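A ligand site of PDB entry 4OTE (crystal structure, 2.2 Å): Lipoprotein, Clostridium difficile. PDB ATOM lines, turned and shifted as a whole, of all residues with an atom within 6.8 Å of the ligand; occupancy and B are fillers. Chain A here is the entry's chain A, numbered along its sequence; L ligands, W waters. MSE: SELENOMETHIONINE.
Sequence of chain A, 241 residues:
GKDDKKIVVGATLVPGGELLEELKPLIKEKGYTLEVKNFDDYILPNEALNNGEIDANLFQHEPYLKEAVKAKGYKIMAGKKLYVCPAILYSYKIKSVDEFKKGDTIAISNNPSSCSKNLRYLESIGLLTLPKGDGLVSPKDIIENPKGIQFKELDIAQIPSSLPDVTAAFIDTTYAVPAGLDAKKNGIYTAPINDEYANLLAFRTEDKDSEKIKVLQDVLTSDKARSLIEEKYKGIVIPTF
O of the ligand sits close to OD1 of Asn 199, at 3.0 Å.
The side-chain hydroxyl (OG1) of Thr 174 is in hydrogen-bond range of a nitrogen (N) of the ligand, 3.5 Å away.
ND2 of Asn 199 is in hydrogen-bond range of O of Phe 59.
OG1 of Thr 174 sits at hydrogen-bond distance from O of Val 14, 2.7 Å away.
The backbone carbonyl oxygen (O) of Tyr 83 is in hydrogen-bond range of the backbone NH (N) of Asn 199, at 2.6 Å.
The backbone NH (N) of Tyr 64 lies within hydrogen-bond range of a ring nitrogen (ND1) of His 61 (3.3 Å).
OH of Tyr 42 is in hydrogen-bond range of OD2 of Asp 172, at 2.6 Å.
O of Tyr 42 is in hydrogen-bond range of OH of Tyr 64.
OD1 of Asn 199 sits close to O of Tyr 197 (3.5 Å).
Residues that only touch the ligand: Phe 59, Tyr 42, Asp 172, Tyr 64, His 61, Cys 85 and Gln 60.
Hydrophobic or aromatic side chains that line the ligand: Tyr 42, Phe 59, His 61 and Tyr 64.
Nine residues have an atom within 4 Å of the ligand: Tyr 42, Phe 59, Gln 60, His 61, Tyr 64, Cys 85, Asp 172, Thr 174 and Asn 199.
Water W1 lies within hydrogen-bond range of O of Tyr 197 (2.7 Å), N of Cys 85 (2.8 Å) and O of the ligand (2.8 Å).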
ATOM      1  N   THR A  12     -18.403   3.389 -10.170  1.00  0.00           N
ATOM      2  CA  THR A  12     -17.445   2.305 -10.054  1.00  0.00           C
ATOM      3  C   THR A  12     -16.788   2.126 -11.421  1.00  0.00           C
ATOM      4  O   THR A  12     -17.422   2.371 -12.445  1.00  0.00           O
ATOM      5  CB  THR A  12     -18.141   1.002  -9.618  1.00  0.00           C
ATOM      6  OG1 THR A  12     -19.346   0.839 -10.366  1.00  0.00           O
ATOM      7  CG2 THR A  12     -18.477   1.066  -8.145  1.00  0.00           C
ATOM      8  N   VAL A  14     -15.859  -0.436 -13.287  1.00  0.00           N
ATOM      9  CA  VAL A  14     -16.439  -1.430 -14.190  1.00  0.00           C
ATOM     10  C   VAL A  14     -17.919  -1.656 -13.851  1.00  0.00           C
ATOM     11  O   VAL A  14     -18.248  -1.975 -12.710  1.00  0.00           O
ATOM     12  CB  VAL A  14     -15.688  -2.772 -14.102  1.00  0.00           C
ATOM     13  CG1 VAL A  14     -16.372  -3.828 -14.953  1.00  0.00           C
ATOM     14  CG2 VAL A  14     -14.243  -2.577 -14.530  1.00  0.00           C
ATOM     15  N   PRO A  15     -18.820  -1.502 -14.844  1.00  0.00           N
ATOM     16  CA  PRO A  15     -18.597  -1.057 -16.220  1.00  0.00           C
ATOM     17  C   PRO A  15     -18.825   0.447 -16.455  1.00  0.00           C
ATOM     18  O   PRO A  15     -18.439   0.973 -17.481  1.00  0.00           O
ATOM     19  CB  PRO A  15     -19.619  -1.860 -17.017  1.00  0.00           C
ATOM     20  CG  PRO A  15     -20.711  -2.170 -16.048  1.00  0.00           C
ATOM     21  CD  PRO A  15     -20.205  -1.947 -14.647  1.00  0.00           C
ATOM     22  N   TYR A  42     -20.272   0.427  -2.796  1.00  0.00           N
ATOM     23  CA  TYR A  42     -21.677   0.691  -3.127  1.00  0.00           C
ATOM     24  C   TYR A  42     -22.380   1.684  -2.188  1.00  0.00           C
ATOM     25  O   TYR A  42     -23.554   1.987  -2.395  1.00  0.00           O
ATOM     26  CB  TYR A  42     -22.462  -0.626  -3.133  1.00  0.00           C
ATOM     27  CG  TYR A  42     -22.112  -1.624  -4.225  1.00  0.00           C
ATOM     28  CD1 TYR A  42     -21.519  -1.222  -5.429  1.00  0.00           C
ATOM     29  CD2 TYR A  42     -22.432  -2.970  -4.083  1.00  0.00           C
ATOM     30  CE1 TYR A  42     -21.232  -2.138  -6.424  1.00  0.00           C
ATOM     31  CE2 TYR A  42     -22.153  -3.892  -5.075  1.00  0.00           C
ATOM     32  CZ  TYR A  42     -21.550  -3.471  -6.243  1.00  0.00           C
ATOM     33  OH  TYR A  42     -21.263  -4.387  -7.238  1.00  0.00           O
ATOM     34  N   PHE A  59     -23.724   3.084 -10.984  1.00  0.00           N
ATOM     35  CA  PHE A  59     -23.213   1.869 -10.327  1.00  0.00           C
ATOM     36  C   PHE A  59     -24.289   0.867  -9.891  1.00  0.00           C
ATOM     37  O   PHE A  59     -23.971  -0.304  -9.671  1.00  0.00           O
ATOM     38  CB  PHE A  59     -22.337   2.249  -9.117  1.00  0.00           C
ATOM     39  CG  PHE A  59     -23.121   2.616  -7.884  1.00  0.00           C
ATOM     40  CD1 PHE A  59     -23.780   3.839  -7.800  1.00  0.00           C
ATOM     41  CD2 PHE A  59     -23.216   1.732  -6.819  1.00  0.00           C
ATOM     42  CE1 PHE A  59     -24.511   4.172  -6.671  1.00  0.00           C
ATOM     43  CE2 PHE A  59     -23.941   2.058  -5.685  1.00  0.00           C
ATOM     44  CZ  PHE A  59     -24.591   3.281  -5.613  1.00  0.00           C
ATOM     45  N   GLN A  60     -25.538   1.313  -9.757  1.00  0.00           N
ATOM     46  CA  GLN A  60     -26.582   0.511  -9.110  1.00  0.00           C
ATOM     47  C   GLN A  60     -27.790   0.245 -10.007  1.00  0.00           C
ATOM     48  O   GLN A  60     -27.964   0.889 -11.056  1.00  0.00           O
ATOM     49  CB  GLN A  60     -27.067   1.224  -7.848  1.00  0.00           C
ATOM     50  CG  GLN A  60     -27.978   2.400  -8.119  1.00  0.00           C
ATOM     51  CD  GLN A  60     -28.024   3.375  -6.964  1.00  0.00           C
ATOM     52  OE1 GLN A  60     -28.389   3.002  -5.852  1.00  0.00           O
ATOM     53  NE2 GLN A  60     -27.653   4.635  -7.215  1.00  0.00           N
ATOM     54  N   HIS A  61     -28.631  -0.700  -9.586  1.00  0.00           N
ATOM     55  CA  HIS A  61     -29.943  -0.905 -10.178  1.00  0.00           C
ATOM     56  C   HIS A  61     -31.016  -0.313  -9.253  1.00  0.00           C
ATOM     57  O   HIS A  61     -30.736   0.086  -8.115  1.00  0.00           O
ATOM     58  CB  HIS A  61     -30.203  -2.395 -10.493  1.00  0.00           C
ATOM     59  CG  HIS A  61     -29.820  -3.350  -9.405  1.00  0.00           C
ATOM     60  ND1 HIS A  61     -30.395  -3.322  -8.152  1.00  0.00           N
ATOM     61  CD2 HIS A  61     -28.960  -4.401  -9.399  1.00  0.00           C
ATOM     62  CE1 HIS A  61     -29.878  -4.290  -7.407  1.00  0.00           C
ATOM     63  NE2 HIS A  61     -29.005  -4.957  -8.141  1.00  0.00           N
ATOM     64  N   TYR A  64     -31.725  -1.708  -5.547  1.00  0.00           N
ATOM     65  CA  TYR A  64     -30.716  -1.291  -4.581  1.00  0.00           C
ATOM     66  C   TYR A  64     -30.952   0.143  -4.157  1.00  0.00           C
ATOM     67  O   TYR A  64     -30.891   0.464  -2.967  1.00  0.00           O
ATOM     68  CB  TYR A  64     -29.307  -1.415  -5.184  1.00  0.00           C
ATOM     69  CG  TYR A  64     -28.216  -1.116  -4.188  1.00  0.00           C
ATOM     70  CD1 TYR A  64     -27.713  -2.104  -3.340  1.00  0.00           C
ATOM     71  CD2 TYR A  64     -27.696   0.178  -4.074  1.00  0.00           C
ATOM     72  CE1 TYR A  64     -26.720  -1.814  -2.427  1.00  0.00           C
ATOM     73  CE2 TYR A  64     -26.703   0.473  -3.153  1.00  0.00           C
ATOM     74  CZ  TYR A  64     -26.217  -0.528  -2.345  1.00  0.00           C
ATOM     75  OH  TYR A  64     -25.223  -0.227  -1.440  1.00  0.00           O
ATOM     76  N   LEU A  65     -31.226   1.018  -5.130  1.00  0.00           N
ATOM     77  CA  LEU A  65     -31.517   2.417  -4.864  1.00  0.00           C
ATOM     78  C   LEU A  65     -32.729   2.559  -3.941  1.00  0.00           C
ATOM     79  O   LEU A  65     -32.678   3.299  -2.953  1.00  0.00           O
ATOM     80  CB  LEU A  65     -31.728   3.185  -6.176  1.00  0.00           C
ATOM     81  CG  LEU A  65     -32.028   4.685  -6.065  1.00  0.00           C
ATOM     82  CD1 LEU A  65     -31.468   5.438  -7.270  1.00  0.00           C
ATOM     83  CD2 LEU A  65     -33.521   4.964  -5.910  1.00  0.00           C
ATOM     84  N   TYR A  83     -28.095  -1.358 -18.709  1.00  0.00           N
ATOM     85  CA  TYR A  83     -27.512  -2.680 -18.926  1.00  0.00           C
ATOM     86  C   TYR A  83     -27.613  -3.539 -17.679  1.00  0.00           C
ATOM     87  O   TYR A  83     -27.646  -3.028 -16.551  1.00  0.00           O
ATOM     88  CB  TYR A  83     -26.037  -2.535 -19.334  1.00  0.00           C
ATOM     89  CG  TYR A  83     -25.247  -1.605 -18.433  1.00  0.00           C
ATOM     90  CD1 TYR A  83     -24.773  -2.028 -17.200  1.00  0.00           C
ATOM     91  CD2 TYR A  83     -24.969  -0.303 -18.833  1.00  0.00           C
ATOM     92  CE1 TYR A  83     -24.057  -1.174 -16.377  1.00  0.00           C
ATOM     93  CE2 TYR A  83     -24.251   0.562 -18.017  1.00  0.00           C
ATOM     94  CZ  TYR A  83     -23.792   0.119 -16.796  1.00  0.00           C
ATOM     95  OH  TYR A  83     -23.082   0.979 -15.978  1.00  0.00           O
ATOM     96  N   VAL A  84     -27.673  -4.852 -17.896  1.00  0.00           N
ATOM     97  CA  VAL A  84     -27.711  -5.828 -16.819  1.00  0.00           C
ATOM     98  C   VAL A  84     -26.326  -6.426 -16.642  1.00  0.00           C
ATOM     99  O   VAL A  84     -25.588  -6.587 -17.616  1.00  0.00           O
ATOM    100  CB  VAL A  84     -28.704  -6.955 -17.118  1.00  0.00           C
ATOM    101  CG1 VAL A  84     -28.982  -7.758 -15.860  1.00  0.00           C
ATOM    102  CG2 VAL A  84     -30.010  -6.398 -17.672  1.00  0.00           C
ATOM    103  N   CYS A  85     -25.983  -6.766 -15.398  1.00  0.00           N
ATOM    104  CA  CYS A  85     -24.727  -7.388 -15.054  1.00  0.00           C
ATOM    105  C   CYS A  85     -25.050  -8.658 -14.270  1.00  0.00           C
ATOM    106  O   CYS A  85     -24.967  -8.650 -13.032  1.00  0.00           O
ATOM    107  CB  CYS A  85     -23.871  -6.435 -14.209  1.00  0.00           C
ATOM    108  SG  CYS A  85     -23.453  -4.856 -15.006  1.00  0.00           S
ATOM    109  N   PRO A  86     -25.454  -9.733 -14.970  1.00  0.00           N
ATOM    110  CA  PRO A  86     -25.862 -10.943 -14.275  1.00  0.00           C
ATOM    111  C   PRO A  86     -24.787 -11.429 -13.315  1.00  0.00           C
ATOM    112  O   PRO A  86     -23.607 -11.411 -13.660  1.00  0.00           O
ATOM    113  CB  PRO A  86     -26.058 -11.958 -15.402  1.00  0.00           C
ATOM    114  CG  PRO A  86     -26.263 -11.157 -16.628  1.00  0.00           C
ATOM    115  CD  PRO A  86     -25.491  -9.892 -16.430  1.00  0.00           C
ATOM    116  N   ALA A  87     -25.193 -11.847 -12.122  1.00  0.00           N
ATOM    117  CA  ALA A  87     -24.276 -12.452 -11.163  1.00  0.00           C
ATOM    118  C   ALA A  87     -23.652 -13.683 -11.781  1.00  0.00           C
ATOM    119  O   ALA A  87     -24.325 -14.466 -12.443  1.00  0.00           O
ATOM    120  CB  ALA A  87     -25.019 -12.817  -9.877  1.00  0.00           C
ATOM    121  N   SER A 114     -28.787  -9.554  -1.888  1.00  0.00           N
ATOM    122  CA  SER A 114     -27.858 -10.336  -2.735  1.00  0.00           C
ATOM    123  C   SER A 114     -27.788 -11.785  -2.290  1.00  0.00           C
ATOM    124  O   SER A 114     -27.828 -12.701  -3.125  1.00  0.00           O
ATOM    125  CB  SER A 114     -26.456  -9.732  -2.698  1.00  0.00           C
ATOM    126  OG  SER A 114     -26.472  -8.348  -3.043  1.00  0.00           O
ATOM    127  N   LYS A 117     -31.039 -13.533  -3.163  1.00  0.00           N
ATOM    128  CA  LYS A 117     -31.101 -13.703  -4.605  1.00  0.00           C
ATOM    129  C   LYS A 117     -30.162 -14.814  -5.094  1.00  0.00           C
ATOM    130  O   LYS A 117     -30.518 -15.604  -5.959  1.00  0.00           O
ATOM    131  CB  LYS A 117     -30.758 -12.375  -5.284  1.00  0.00           C
ATOM    132  CG  LYS A 117     -30.964 -12.369  -6.784  1.00  0.00           C
ATOM    133  CD  LYS A 117     -31.140 -10.958  -7.321  1.00  0.00           C
ATOM    134  CE  LYS A 117     -30.019 -10.023  -6.898  1.00  0.00           C
ATOM    135  NZ  LYS A 117     -30.270  -8.637  -7.367  1.00  0.00           N
ATOM    136  N   ILE A 156     -18.654  -7.945   0.553  1.00  0.00           N
ATOM    137  CA  ILE A 156     -18.504  -8.058  -0.894  1.00  0.00           C
ATOM    138  C   ILE A 156     -17.064  -7.846  -1.380  1.00  0.00           C
ATOM    139  O   ILE A 156     -16.629  -8.497  -2.322  1.00  0.00           O
ATOM    140  CB  ILE A 156     -19.472  -7.098  -1.636  1.00  0.00           C
ATOM    141  CG1 ILE A 156     -19.470  -7.389  -3.142  1.00  0.00           C
ATOM    142  CG2 ILE A 156     -19.124  -5.645  -1.362  1.00  0.00           C
ATOM    143  CD1 ILE A 156     -20.635  -6.750  -3.861  1.00  0.00           C
ATOM    144  N   ASP A 172     -20.040  -9.922  -8.108  1.00  0.00           N
ATOM    145  CA  ASP A 172     -20.482  -8.864  -9.005  1.00  0.00           C
ATOM    146  C   ASP A 172     -19.404  -8.564 -10.039  1.00  0.00           C
ATOM    147  O   ASP A 172     -18.207  -8.560  -9.722  1.00  0.00           O
ATOM    148  CB  ASP A 172     -20.801  -7.578  -8.233  1.00  0.00           C
ATOM    149  CG  ASP A 172     -22.037  -7.684  -7.373  1.00  0.00           C
ATOM    150  OD1 ASP A 172     -22.462  -8.829  -7.079  1.00  0.00           O
ATOM    151  OD2 ASP A 172     -22.583  -6.636  -6.979  1.00  0.00           O
ATOM    152  N   THR A 173     -19.819  -8.314 -11.270  1.00  0.00           N
ATOM    153  CA  THR A 173     -18.871  -7.992 -12.339  1.00  0.00           C
ATOM    154  C   THR A 173     -18.056  -6.743 -11.976  1.00  0.00           C
ATOM    155  O   THR A 173     -16.867  -6.675 -12.303  1.00  0.00           O
ATOM    156  CB  THR A 173     -19.602  -7.875 -13.693  1.00  0.00           C
ATOM    157  OG1 THR A 173     -19.917  -9.191 -14.150  1.00  0.00           O
ATOM    158  CG2 THR A 173     -18.748  -7.164 -14.755  1.00  0.00           C
ATOM    159  N   THR A 174     -18.680  -5.785 -11.290  1.00  0.00           N
ATOM    160  CA  THR A 174     -17.988  -4.600 -10.782  1.00  0.00           C
ATOM    161  C   THR A 174     -16.748  -4.954  -9.922  1.00  0.00           C
ATOM    162  O   THR A 174     -15.751  -4.239  -9.950  1.00  0.00           O
ATOM    163  CB  THR A 174     -18.945  -3.686  -9.969  1.00  0.00           C
ATOM    164  OG1 THR A 174     -19.898  -3.090 -10.867  1.00  0.00           O
ATOM    165  CG2 THR A 174     -18.197  -2.569  -9.253  1.00  0.00           C
ATOM    166  N   TYR A 197     -33.005  -5.737 -12.622  1.00  0.00           N
ATOM    167  CA  TYR A 197     -31.691  -5.454 -12.052  1.00  0.00           C
ATOM    168  C   TYR A 197     -30.768  -4.726 -13.026  1.00  0.00           C
ATOM    169  O   TYR A 197     -29.539  -4.755 -12.873  1.00  0.00           O
ATOM    170  CB  TYR A 197     -31.058  -6.765 -11.572  1.00  0.00           C
ATOM    171  CG  TYR A 197     -31.908  -7.479 -10.543  1.00  0.00           C
ATOM    172  CD1 TYR A 197     -32.267  -6.837  -9.356  1.00  0.00           C
ATOM    173  CD2 TYR A 197     -32.361  -8.781 -10.740  1.00  0.00           C
ATOM    174  CE1 TYR A 197     -33.057  -7.460  -8.411  1.00  0.00           C
ATOM    175  CE2 TYR A 197     -33.145  -9.416  -9.798  1.00  0.00           C
ATOM    176  CZ  TYR A 197     -33.485  -8.755  -8.633  1.00  0.00           C
ATOM    177  OH  TYR A 197     -34.261  -9.362  -7.684  1.00  0.00           O
ATOM    178  N   ALA A 198     -31.340  -4.052 -14.020  1.00  0.00           N
ATOM    179  CA  ALA A 198     -30.554  -3.251 -14.944  1.00  0.00           C
ATOM    180  C   ALA A 198     -29.907  -2.084 -14.196  1.00  0.00           C
ATOM    181  O   ALA A 198     -30.580  -1.347 -13.476  1.00  0.00           O
ATOM    182  CB  ALA A 198     -31.428  -2.733 -16.069  1.00  0.00           C
ATOM    183  N   ASN A 199     -28.587  -1.953 -14.340  1.00  0.00           N
ATOM    184  CA  ASN A 199     -27.892  -0.794 -13.805  1.00  0.00           C
ATOM    185  C   ASN A 199     -28.324   0.438 -14.571  1.00  0.00           C
ATOM    186  O   ASN A 199     -28.750   0.340 -15.737  1.00  0.00           O
ATOM    187  CB  ASN A 199     -26.371  -0.959 -13.897  1.00  0.00           C
ATOM    188  CG  ASN A 199     -25.841  -2.036 -12.970  1.00  0.00           C
ATOM    189  OD1 ASN A 199     -26.553  -2.978 -12.610  1.00  0.00           O
ATOM    190  ND2 ASN A 199     -24.580  -1.908 -12.581  1.00  0.00           N
HETATM  191  N   MSE L   1     -23.182  -4.173 -11.042  1.00  0.00           N
HETATM  192  CA  MSE L   1     -23.923  -4.675  -9.849  1.00  0.00           C
HETATM  193  C   MSE L   1     -24.905  -5.709 -10.295  1.00  0.00           C
HETATM  194  O   MSE L   1     -25.743  -5.442 -11.163  1.00  0.00           O
HETATM  195  OXT MSE L   1     -24.864  -6.831  -9.778  1.00  0.00           O
HETATM  196  CB  MSE L   1     -24.674  -3.581  -9.102  1.00  0.00           C
HETATM  197  CG  MSE L   1     -25.294  -4.095  -7.799  1.00  0.00           C
HETATM  198 SE   MSE L   1     -26.422  -2.709  -6.954  1.00  0.00          SE
HETATM  199  CE  MSE L   1     -24.962  -1.542  -6.361  1.00  0.00           C
HETATM  200  O   HOH W   1     -27.497  -6.455 -13.096  1.00  0.00           O
